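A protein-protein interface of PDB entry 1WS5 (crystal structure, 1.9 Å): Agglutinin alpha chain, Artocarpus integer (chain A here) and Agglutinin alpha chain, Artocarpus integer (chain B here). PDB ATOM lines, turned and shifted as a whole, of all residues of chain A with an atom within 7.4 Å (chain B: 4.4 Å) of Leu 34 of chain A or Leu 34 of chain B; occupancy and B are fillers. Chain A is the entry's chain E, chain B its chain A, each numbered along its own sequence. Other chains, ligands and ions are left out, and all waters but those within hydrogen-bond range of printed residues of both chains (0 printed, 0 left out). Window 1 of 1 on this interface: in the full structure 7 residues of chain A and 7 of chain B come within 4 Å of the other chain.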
ATOM      1  N   ASP A   6      27.996  -8.320  -5.125  1.00  0.00           N
ATOM      2  CA  ASP A   6      26.984  -9.337  -5.395  1.00  0.00           C
ATOM      3  C   ASP A   6      27.565 -10.744  -5.476  1.00  0.00           C
ATOM      4  O   ASP A   6      26.895 -11.719  -5.138  1.00  0.00           O
ATOM      5  CB  ASP A   6      26.243  -9.035  -6.700  1.00  0.00           C
ATOM      6  CG  ASP A   6      25.303  -7.851  -6.583  1.00  0.00           C
ATOM      7  OD1 ASP A   6      25.037  -7.403  -5.446  1.00  0.00           O
ATOM      8  OD2 ASP A   6      24.822  -7.379  -7.629  1.00  0.00           O
ATOM      9  N   GLY A   7      28.810 -10.848  -5.926  1.00  0.00           N
ATOM     10  CA  GLY A   7      29.428 -12.153  -6.052  1.00  0.00           C
ATOM     11  C   GLY A   7      29.226 -12.645  -7.470  1.00  0.00           C
ATOM     12  O   GLY A   7      28.779 -11.888  -8.331  1.00  0.00           O
ATOM     13  N   ALA A   8      29.538 -13.912  -7.715  1.00  0.00           N
ATOM     14  CA  ALA A   8      29.397 -14.477  -9.050  1.00  0.00           C
ATOM     15  C   ALA A   8      28.210 -15.427  -9.146  1.00  0.00           C
ATOM     16  O   ALA A   8      27.899 -16.149  -8.203  1.00  0.00           O
ATOM     17  CB  ALA A   8      30.670 -15.208  -9.442  1.00  0.00           C
ATOM     18  N   PHE A   9      27.553 -15.414 -10.299  1.00  0.00           N
ATOM     19  CA  PHE A   9      26.411 -16.283 -10.535  1.00  0.00           C
ATOM     20  C   PHE A   9      26.645 -17.013 -11.851  1.00  0.00           C
ATOM     21  O   PHE A   9      27.779 -17.097 -12.313  1.00  0.00           O
ATOM     22  CB  PHE A   9      25.120 -15.462 -10.569  1.00  0.00           C
ATOM     23  CG  PHE A   9      24.809 -14.786  -9.262  1.00  0.00           C
ATOM     24  CD1 PHE A   9      25.482 -13.630  -8.884  1.00  0.00           C
ATOM     25  CD2 PHE A   9      23.884 -15.340  -8.381  1.00  0.00           C
ATOM     26  CE1 PHE A   9      25.239 -13.032  -7.645  1.00  0.00           C
ATOM     27  CE2 PHE A   9      23.634 -14.750  -7.139  1.00  0.00           C
ATOM     28  CZ  PHE A   9      24.316 -13.594  -6.773  1.00  0.00           C
ATOM     29  N   THR A  10      25.595 -17.547 -12.463  1.00  0.00           N
ATOM     30  CA  THR A  10      25.795 -18.272 -13.710  1.00  0.00           C
ATOM     31  C   THR A  10      25.402 -17.506 -14.966  1.00  0.00           C
ATOM     32  O   THR A  10      25.608 -17.988 -16.077  1.00  0.00           O
ATOM     33  CB  THR A  10      25.076 -19.642 -13.669  1.00  0.00           C
ATOM     34  OG1 THR A  10      23.780 -19.491 -13.087  1.00  0.00           O
ATOM     35  CG2 THR A  10      25.877 -20.633 -12.823  1.00  0.00           C
ATOM     36  N   GLY A  11      24.861 -16.304 -14.786  1.00  0.00           N
ATOM     37  CA  GLY A  11      24.468 -15.487 -15.920  1.00  0.00           C
ATOM     38  C   GLY A  11      23.732 -14.231 -15.492  1.00  0.00           C
ATOM     39  O   GLY A  11      23.527 -14.002 -14.302  1.00  0.00           O
ATOM     40  N   ILE A  12      23.342 -13.409 -16.463  1.00  0.00           N
ATOM     41  CA  ILE A  12      22.618 -12.174 -16.175  1.00  0.00           C
ATOM     42  C   ILE A  12      21.284 -12.190 -16.917  1.00  0.00           C
ATOM     43  O   ILE A  12      21.236 -12.471 -18.115  1.00  0.00           O
ATOM     44  CB  ILE A  12      23.385 -10.917 -16.653  1.00  0.00           C
ATOM     45  CG1 ILE A  12      24.817 -10.913 -16.110  1.00  0.00           C
ATOM     46  CG2 ILE A  12      22.635  -9.658 -16.202  1.00  0.00           C
ATOM     47  CD1 ILE A  12      24.912 -10.765 -14.628  1.00  0.00           C
ATOM     48  N   ARG A  13      20.208 -11.874 -16.205  1.00  0.00           N
ATOM     49  CA  ARG A  13      18.880 -11.848 -16.802  1.00  0.00           C
ATOM     50  C   ARG A  13      18.357 -10.433 -17.012  1.00  0.00           C
ATOM     51  O   ARG A  13      17.755 -10.132 -18.040  1.00  0.00           O
ATOM     52  CB  ARG A  13      17.897 -12.622 -15.923  1.00  0.00           C
ATOM     53  CG  ARG A  13      18.050 -14.136 -16.016  1.00  0.00           C
ATOM     54  CD  ARG A  13      17.227 -14.839 -14.951  1.00  0.00           C
ATOM     55  NE  ARG A  13      17.299 -16.292 -15.084  1.00  0.00           N
ATOM     56  CZ  ARG A  13      16.459 -17.021 -15.812  1.00  0.00           C
ATOM     57  NH1 ARG A  13      15.469 -16.441 -16.476  1.00  0.00           N
ATOM     58  NH2 ARG A  13      16.618 -18.336 -15.885  1.00  0.00           N
ATOM     59  N   VAL A  31      19.333  -8.791 -11.767  1.00  0.00           N
ATOM     60  CA  VAL A  31      18.629 -10.048 -11.549  1.00  0.00           C
ATOM     61  C   VAL A  31      19.529 -11.044 -12.263  1.00  0.00           C
ATOM     62  O   VAL A  31      19.672 -11.001 -13.486  1.00  0.00           O
ATOM     63  CB  VAL A  31      17.237 -10.083 -12.207  1.00  0.00           C
ATOM     64  CG1 VAL A  31      16.612 -11.464 -12.005  1.00  0.00           C
ATOM     65  CG2 VAL A  31      16.343  -9.022 -11.596  1.00  0.00           C
ATOM     66  N   TYR A  32      20.160 -11.920 -11.497  1.00  0.00           N
ATOM     67  CA  TYR A  32      21.059 -12.902 -12.074  1.00  0.00           C
ATOM     68  C   TYR A  32      20.368 -14.219 -12.341  1.00  0.00           C
ATOM     69  O   TYR A  32      19.227 -14.440 -11.932  1.00  0.00           O
ATOM     70  CB  TYR A  32      22.220 -13.198 -11.123  1.00  0.00           C
ATOM     71  CG  TYR A  32      23.071 -12.011 -10.772  1.00  0.00           C
ATOM     72  CD1 TYR A  32      22.786 -11.228  -9.652  1.00  0.00           C
ATOM     73  CD2 TYR A  32      24.166 -11.668 -11.561  1.00  0.00           C
ATOM     74  CE1 TYR A  32      23.578 -10.131  -9.325  1.00  0.00           C
ATOM     75  CE2 TYR A  32      24.961 -10.573 -11.246  1.00  0.00           C
ATOM     76  CZ  TYR A  32      24.666  -9.811 -10.130  1.00  0.00           C
ATOM     77  OH  TYR A  32      25.465  -8.734  -9.817  1.00  0.00           O
ATOM     78  N   ASP A  33      21.075 -15.091 -13.047  1.00  0.00           N
ATOM     79  CA  ASP A  33      20.571 -16.429 -13.268  1.00  0.00           C
ATOM     80  C   ASP A  33      21.383 -17.252 -12.286  1.00  0.00           C
ATOM     81  O   ASP A  33      22.584 -17.034 -12.132  1.00  0.00           O
ATOM     82  CB  ASP A  33      20.864 -16.951 -14.667  1.00  0.00           C
ATOM     83  CG  ASP A  33      20.395 -18.382 -14.840  1.00  0.00           C
ATOM     84  OD1 ASP A  33      19.168 -18.595 -14.904  1.00  0.00           O
ATOM     85  OD2 ASP A  33      21.246 -19.295 -14.880  1.00  0.00           O
ATOM     86  N   LEU A  34      20.726 -18.173 -11.600  1.00  0.00           N
ATOM     87  CA  LEU A  34      21.417 -19.039 -10.667  1.00  0.00           C
ATOM     88  C   LEU A  34      21.029 -20.457 -11.042  1.00  0.00           C
ATOM     89  O   LEU A  34      20.001 -20.966 -10.600  1.00  0.00           O
ATOM     90  CB  LEU A  34      20.999 -18.749  -9.225  1.00  0.00           C
ATOM     91  CG  LEU A  34      21.644 -19.651  -8.163  1.00  0.00           C
ATOM     92  CD1 LEU A  34      23.162 -19.532  -8.217  1.00  0.00           C
ATOM     93  CD2 LEU A  34      21.130 -19.263  -6.790  1.00  0.00           C
ATOM     94  N   ASN A  35      21.840 -21.073 -11.891  1.00  0.00           N
ATOM     95  CA  ASN A  35      21.591 -22.439 -12.316  1.00  0.00           C
ATOM     96  C   ASN A  35      20.208 -22.620 -12.953  1.00  0.00           C
ATOM     97  O   ASN A  35      19.509 -23.595 -12.673  1.00  0.00           O
ATOM     98  CB  ASN A  35      21.753 -23.371 -11.111  1.00  0.00           C
ATOM     99  CG  ASN A  35      23.136 -23.269 -10.479  1.00  0.00           C
ATOM    100  OD1 ASN A  35      23.268 -23.115  -9.261  1.00  0.00           O
ATOM    101  ND2 ASN A  35      24.174 -23.358 -11.304  1.00  0.00           N
ATOM    102  N   GLY A  36      19.815 -21.675 -13.804  1.00  0.00           N
ATOM    103  CA  GLY A  36      18.534 -21.787 -14.483  1.00  0.00           C
ATOM    104  C   GLY A  36      17.351 -21.064 -13.871  1.00  0.00           C
ATOM    105  O   GLY A  36      16.288 -20.979 -14.491  1.00  0.00           O
ATOM    106  N   SER A  37      17.510 -20.558 -12.657  1.00  0.00           N
ATOM    107  CA  SER A  37      16.428 -19.836 -12.001  1.00  0.00           C
ATOM    108  C   SER A  37      16.855 -18.406 -11.722  1.00  0.00           C
ATOM    109  O   SER A  37      18.027 -18.140 -11.455  1.00  0.00           O
ATOM    110  CB  SER A  37      16.043 -20.517 -10.688  1.00  0.00           C
ATOM    111  OG  SER A  37      15.488 -21.800 -10.928  1.00  0.00           O
ATOM    112  N   PRO A  38      15.908 -17.463 -11.791  1.00  0.00           N
ATOM    113  CA  PRO A  38      16.221 -16.056 -11.536  1.00  0.00           C
ATOM    114  C   PRO A  38      16.611 -15.842 -10.082  1.00  0.00           C
ATOM    115  O   PRO A  38      16.050 -16.467  -9.179  1.00  0.00           O
ATOM    116  CB  PRO A  38      14.913 -15.340 -11.877  1.00  0.00           C
ATOM    117  CG  PRO A  38      14.262 -16.254 -12.876  1.00  0.00           C
ATOM    118  CD  PRO A  38      14.523 -17.610 -12.271  1.00  0.00           C
ATOM    119  N   TYR A  39      17.586 -14.970  -9.860  1.00  0.00           N
ATOM    120  CA  TYR A  39      18.014 -14.650  -8.511  1.00  0.00           C
ATOM    121  C   TYR A  39      18.095 -13.133  -8.436  1.00  0.00           C
ATOM    122  O   TYR A  39      18.914 -12.512  -9.115  1.00  0.00           O
ATOM    123  CB  TYR A  39      19.373 -15.275  -8.194  1.00  0.00           C
ATOM    124  CG  TYR A  39      19.818 -15.018  -6.776  1.00  0.00           C
ATOM    125  CD1 TYR A  39      20.435 -13.816  -6.427  1.00  0.00           C
ATOM    126  CD2 TYR A  39      19.583 -15.952  -5.770  1.00  0.00           C
ATOM    127  CE1 TYR A  39      20.806 -13.551  -5.115  1.00  0.00           C
ATOM    128  CE2 TYR A  39      19.949 -15.693  -4.450  1.00  0.00           C
ATOM    129  CZ  TYR A  39      20.561 -14.488  -4.133  1.00  0.00           C
ATOM    130  OH  TYR A  39      20.927 -14.217  -2.835  1.00  0.00           O
ATOM    131  N   PHE A  60      17.565 -13.869 -21.998  1.00  0.00           N
ATOM    132  CA  PHE A  60      18.406 -14.942 -21.477  1.00  0.00           C
ATOM    133  C   PHE A  60      17.831 -16.293 -21.925  1.00  0.00           C
ATOM    134  O   PHE A  60      16.620 -16.494 -21.889  1.00  0.00           O
ATOM    135  CB  PHE A  60      18.421 -14.868 -19.945  1.00  0.00           C
ATOM    136  CG  PHE A  60      19.277 -15.913 -19.291  1.00  0.00           C
ATOM    137  CD1 PHE A  60      20.661 -15.767 -19.240  1.00  0.00           C
ATOM    138  CD2 PHE A  60      18.701 -17.054 -18.742  1.00  0.00           C
ATOM    139  CE1 PHE A  60      21.458 -16.745 -18.651  1.00  0.00           C
ATOM    140  CE2 PHE A  60      19.491 -18.038 -18.152  1.00  0.00           C
ATOM    141  CZ  PHE A  60      20.873 -17.880 -18.108  1.00  0.00           C
ATOM    142  N   PHE B   9      27.861 -23.585  -7.069  1.00  0.00           N
ATOM    143  CA  PHE B   9      27.785 -22.515  -6.082  1.00  0.00           C
ATOM    144  C   PHE B   9      29.170 -22.028  -5.674  1.00  0.00           C
ATOM    145  O   PHE B   9      30.158 -22.321  -6.347  1.00  0.00           O
ATOM    146  CB  PHE B   9      26.995 -22.978  -4.854  1.00  0.00           C
ATOM    147  CG  PHE B   9      25.565 -23.336  -5.162  1.00  0.00           C
ATOM    148  CD1 PHE B   9      25.247 -24.567  -5.730  1.00  0.00           C
ATOM    149  CD2 PHE B   9      24.541 -22.425  -4.919  1.00  0.00           C
ATOM    150  CE1 PHE B   9      23.928 -24.885  -6.052  1.00  0.00           C
ATOM    151  CE2 PHE B   9      23.217 -22.734  -5.239  1.00  0.00           C
ATOM    152  CZ  PHE B   9      22.912 -23.966  -5.806  1.00  0.00           C
ATOM    153  N   THR B  10      29.233 -21.289  -4.570  1.00  0.00           N
ATOM    154  CA  THR B  10      30.485 -20.722  -4.075  1.00  0.00           C
ATOM    155  C   THR B  10      31.260 -21.664  -3.158  1.00  0.00           C
ATOM    156  O   THR B  10      32.474 -21.532  -3.008  1.00  0.00           O
ATOM    157  CB  THR B  10      30.222 -19.418  -3.285  1.00  0.00           C
ATOM    158  OG1 THR B  10      29.313 -18.590  -4.012  1.00  0.00           O
ATOM    159  CG2 THR B  10      31.517 -18.660  -3.080  1.00  0.00           C
ATOM    160  N   TYR B  32      24.545 -25.006   0.433  1.00  0.00           N
ATOM    161  CA  TYR B  32      25.695 -24.394  -0.211  1.00  0.00           C
ATOM    162  C   TYR B  32      25.952 -22.994   0.287  1.00  0.00           C
ATOM    163  O   TYR B  32      25.135 -22.413   1.003  1.00  0.00           O
ATOM    164  CB  TYR B  32      25.470 -24.281  -1.723  1.00  0.00           C
ATOM    165  CG  TYR B  32      25.267 -25.591  -2.436  1.00  0.00           C
ATOM    166  CD1 TYR B  32      23.986 -26.112  -2.630  1.00  0.00           C
ATOM    167  CD2 TYR B  32      26.358 -26.315  -2.915  1.00  0.00           C
ATOM    168  CE1 TYR B  32      23.797 -27.321  -3.286  1.00  0.00           C
ATOM    169  CE2 TYR B  32      26.180 -27.530  -3.572  1.00  0.00           C
ATOM    170  CZ  TYR B  32      24.901 -28.025  -3.752  1.00  0.00           C
ATOM    171  OH  TYR B  32      24.727 -29.226  -4.397  1.00  0.00           O
ATOM    172  N   ASP B  33      27.108 -22.463  -0.090  1.00  0.00           N
ATOM    173  CA  ASP B  33      27.406 -21.083   0.213  1.00  0.00           C
ATOM    174  C   ASP B  33      27.171 -20.422  -1.131  1.00  0.00           C
ATOM    175  O   ASP B  33      27.541 -20.972  -2.175  1.00  0.00           O
ATOM    176  CB  ASP B  33      28.860 -20.841   0.596  1.00  0.00           C
ATOM    177  CG  ASP B  33      29.151 -19.358   0.788  1.00  0.00           C
ATOM    178  OD1 ASP B  33      28.625 -18.777   1.761  1.00  0.00           O
ATOM    179  OD2 ASP B  33      29.877 -18.765  -0.041  1.00  0.00           O
ATOM    180  N   LEU B  34      26.530 -19.263  -1.112  1.00  0.00           N
ATOM    181  CA  LEU B  34      26.282 -18.518  -2.330  1.00  0.00           C
ATOM    182  C   LEU B  34      26.779 -17.110  -2.058  1.00  0.00           C
ATOM    183  O   LEU B  34      26.047 -16.279  -1.514  1.00  0.00           O
ATOM    184  CB  LEU B  34      24.791 -18.492  -2.672  1.00  0.00           C
ATOM    185  CG  LEU B  34      24.439 -17.673  -3.921  1.00  0.00           C
ATOM    186  CD1 LEU B  34      25.162 -18.251  -5.134  1.00  0.00           C
ATOM    187  CD2 LEU B  34      22.935 -17.680  -4.148  1.00  0.00           C
ATOM    188  N   ASN B  35      28.040 -16.865  -2.391  1.00  0.00           N
ATOM    189  CA  ASN B  35      28.641 -15.551  -2.204  1.00  0.00           C
ATOM    190  C   ASN B  35      28.545 -15.025  -0.772  1.00  0.00           C
ATOM    191  O   ASN B  35      28.179 -13.869  -0.548  1.00  0.00           O
ATOM    192  CB  ASN B  35      27.995 -14.564  -3.183  1.00  0.00           C
ATOM    193  CG  ASN B  35      28.154 -15.000  -4.628  1.00  0.00           C
ATOM    194  OD1 ASN B  35      27.186 -15.044  -5.394  1.00  0.00           O
ATOM    195  ND2 ASN B  35      29.382 -15.326  -5.009  1.00  0.00           N
ATOM    196  N   GLY B  36      28.876 -15.877   0.195  1.00  0.00           N
ATOM    197  CA  GLY B  36      28.851 -15.461   1.586  1.00  0.00           C
ATOM    198  C   GLY B  36      27.607 -15.784   2.389  1.00  0.00           C
ATOM    199  O   GLY B  36      27.636 -15.710   3.617  1.00  0.00           O
ATOM    200  N   SER B  37      26.516 -16.133   1.714  1.00  0.00           N
ATOM    201  CA  SER B  37      25.272 -16.465   2.399  1.00  0.00           C
ATOM    202  C   SER B  37      24.878 -17.913   2.138  1.00  0.00           C
ATOM    203  O   SER B  37      25.135 -18.451   1.060  1.00  0.00           O
ATOM    204  CB  SER B  37      24.137 -15.551   1.930  1.00  0.00           C
ATOM    205  OG  SER B  37      24.413 -14.190   2.224  1.00  0.00           O
ATOM    206  N   TYR B  39      22.753 -21.133   1.136  1.00  0.00           N
ATOM    207  CA  TYR B  39      21.715 -21.364   0.142  1.00  0.00           C
ATOM    208  C   TYR B  39      21.265 -22.808   0.322  1.00  0.00           C
ATOM    209  O   TYR B  39      22.019 -23.740   0.051  1.00  0.00           O
ATOM    210  CB  TYR B  39      22.233 -21.140  -1.280  1.00  0.00           C
ATOM    211  CG  TYR B  39      21.161 -21.335  -2.331  1.00  0.00           C
ATOM    212  CD1 TYR B  39      20.863 -22.603  -2.829  1.00  0.00           C
ATOM    213  CD2 TYR B  39      20.406 -20.255  -2.788  1.00  0.00           C
ATOM    214  CE1 TYR B  39      19.840 -22.791  -3.756  1.00  0.00           C
ATOM    215  CE2 TYR B  39      19.382 -20.433  -3.714  1.00  0.00           C
ATOM    216  CZ  TYR B  39      19.105 -21.701  -4.193  1.00  0.00           C
ATOM    217  OH  TYR B  39      18.089 -21.877  -5.105  1.00  0.00           O
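O of Asp 6 of chain A sits close to OD1 of Asn 35 of chain B (3.3 Å). The side-chain amide nitrogen of Asn 35 of chain B lies close to the backbone NH of Ala 8 of chain A, at 3.1 Å.
OG1 of Thr 10 of chain B sits at hydrogen-bond distance from N of Asn 35 of chain B, 2.7 Å away. The backbone NH (N) of Tyr 39 of chain B sits at hydrogen-bond distance from the backbone carbonyl oxygen (O) of Tyr 32 of chain B. The side-chain hydroxyl (OH) of Tyr 32 of chain A sits at hydrogen-bond distance from the side-chain carboxylate (OD2) of Asp 6 of chain A (2.7 Å). The side-chain hydroxyl (OG1) of Thr 10 of chain A is in hydrogen-bond range of the backbone NH (N) of Asn 35 of chain A (2.8 Å). The backbone carbonyl oxygen (O) of Tyr 32 of chain A lies within hydrogen-bond range of the backbone NH (N) of Tyr 39 of chain A (2.7 Å).
ND2 of Asn 35 of chain B touches CA of Gly 7 of chain A, 3.3 Å away. Phe 9 of chain A touches Asn 35 of chain B. Leu 34 of chain B touches Leu 34 of chain A. Leu 34 of chain A touches Tyr 39 of chain B (CD2 to CE2, 3.7 Å). Phe 9 of chain B touches Asn 35 of chain A. CE2 of Tyr 39 of chain A touches CD2 of Leu 34 of chain B, at 3.6 Å.
Printed residues of chain B within 4 Å of Asp 6 of chain A: Asn 35 (3.3 Å). Printed residues of chain B within 4 Å of Ala 8 of chain A: Asn 35 (3.1 Å). Leu 34 of chain A touches just these residues of chain B: Leu 34 (3.6 Å) and Tyr 39 (3.7 Å). Of the printed residues of chain B, Tyr 39 of chain A touches Leu 34 (3.6 Å). Thr 10 of chain B touches none of the printed residues of chain A. Of chain A, only Leu 34 and Tyr 39 come within 4 Å of Leu 34 of chain B. Printed residues of chain A within 4 Å of Tyr 39 of chain B: Leu 34 (3.7 Å). The nearest residue of chain A that does not touch Leu 34 of chain B is Phe 9 of chain A (4.2 Å). The nearest printed residue of chain A that does not touch Asn 35 of chain B is Tyr 39 of chain A (6.6 Å).
Hydrophobic or aromatic side chains of chain A within 4 Å of the printed part of chain B: Phe 9, Leu 34 and Tyr 39. Of the 9 printed residues of chain B, 4 touch a printed residue of chain A. Printed residues of chain B that touch a printed residue of chain A: Phe 9, Leu 34, Asn 35 and Tyr 39. Among the printed residues, no Asp or Glu carboxylate lies within 4 Å of a Lys or Arg side-chain nitrogen of the other chain.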
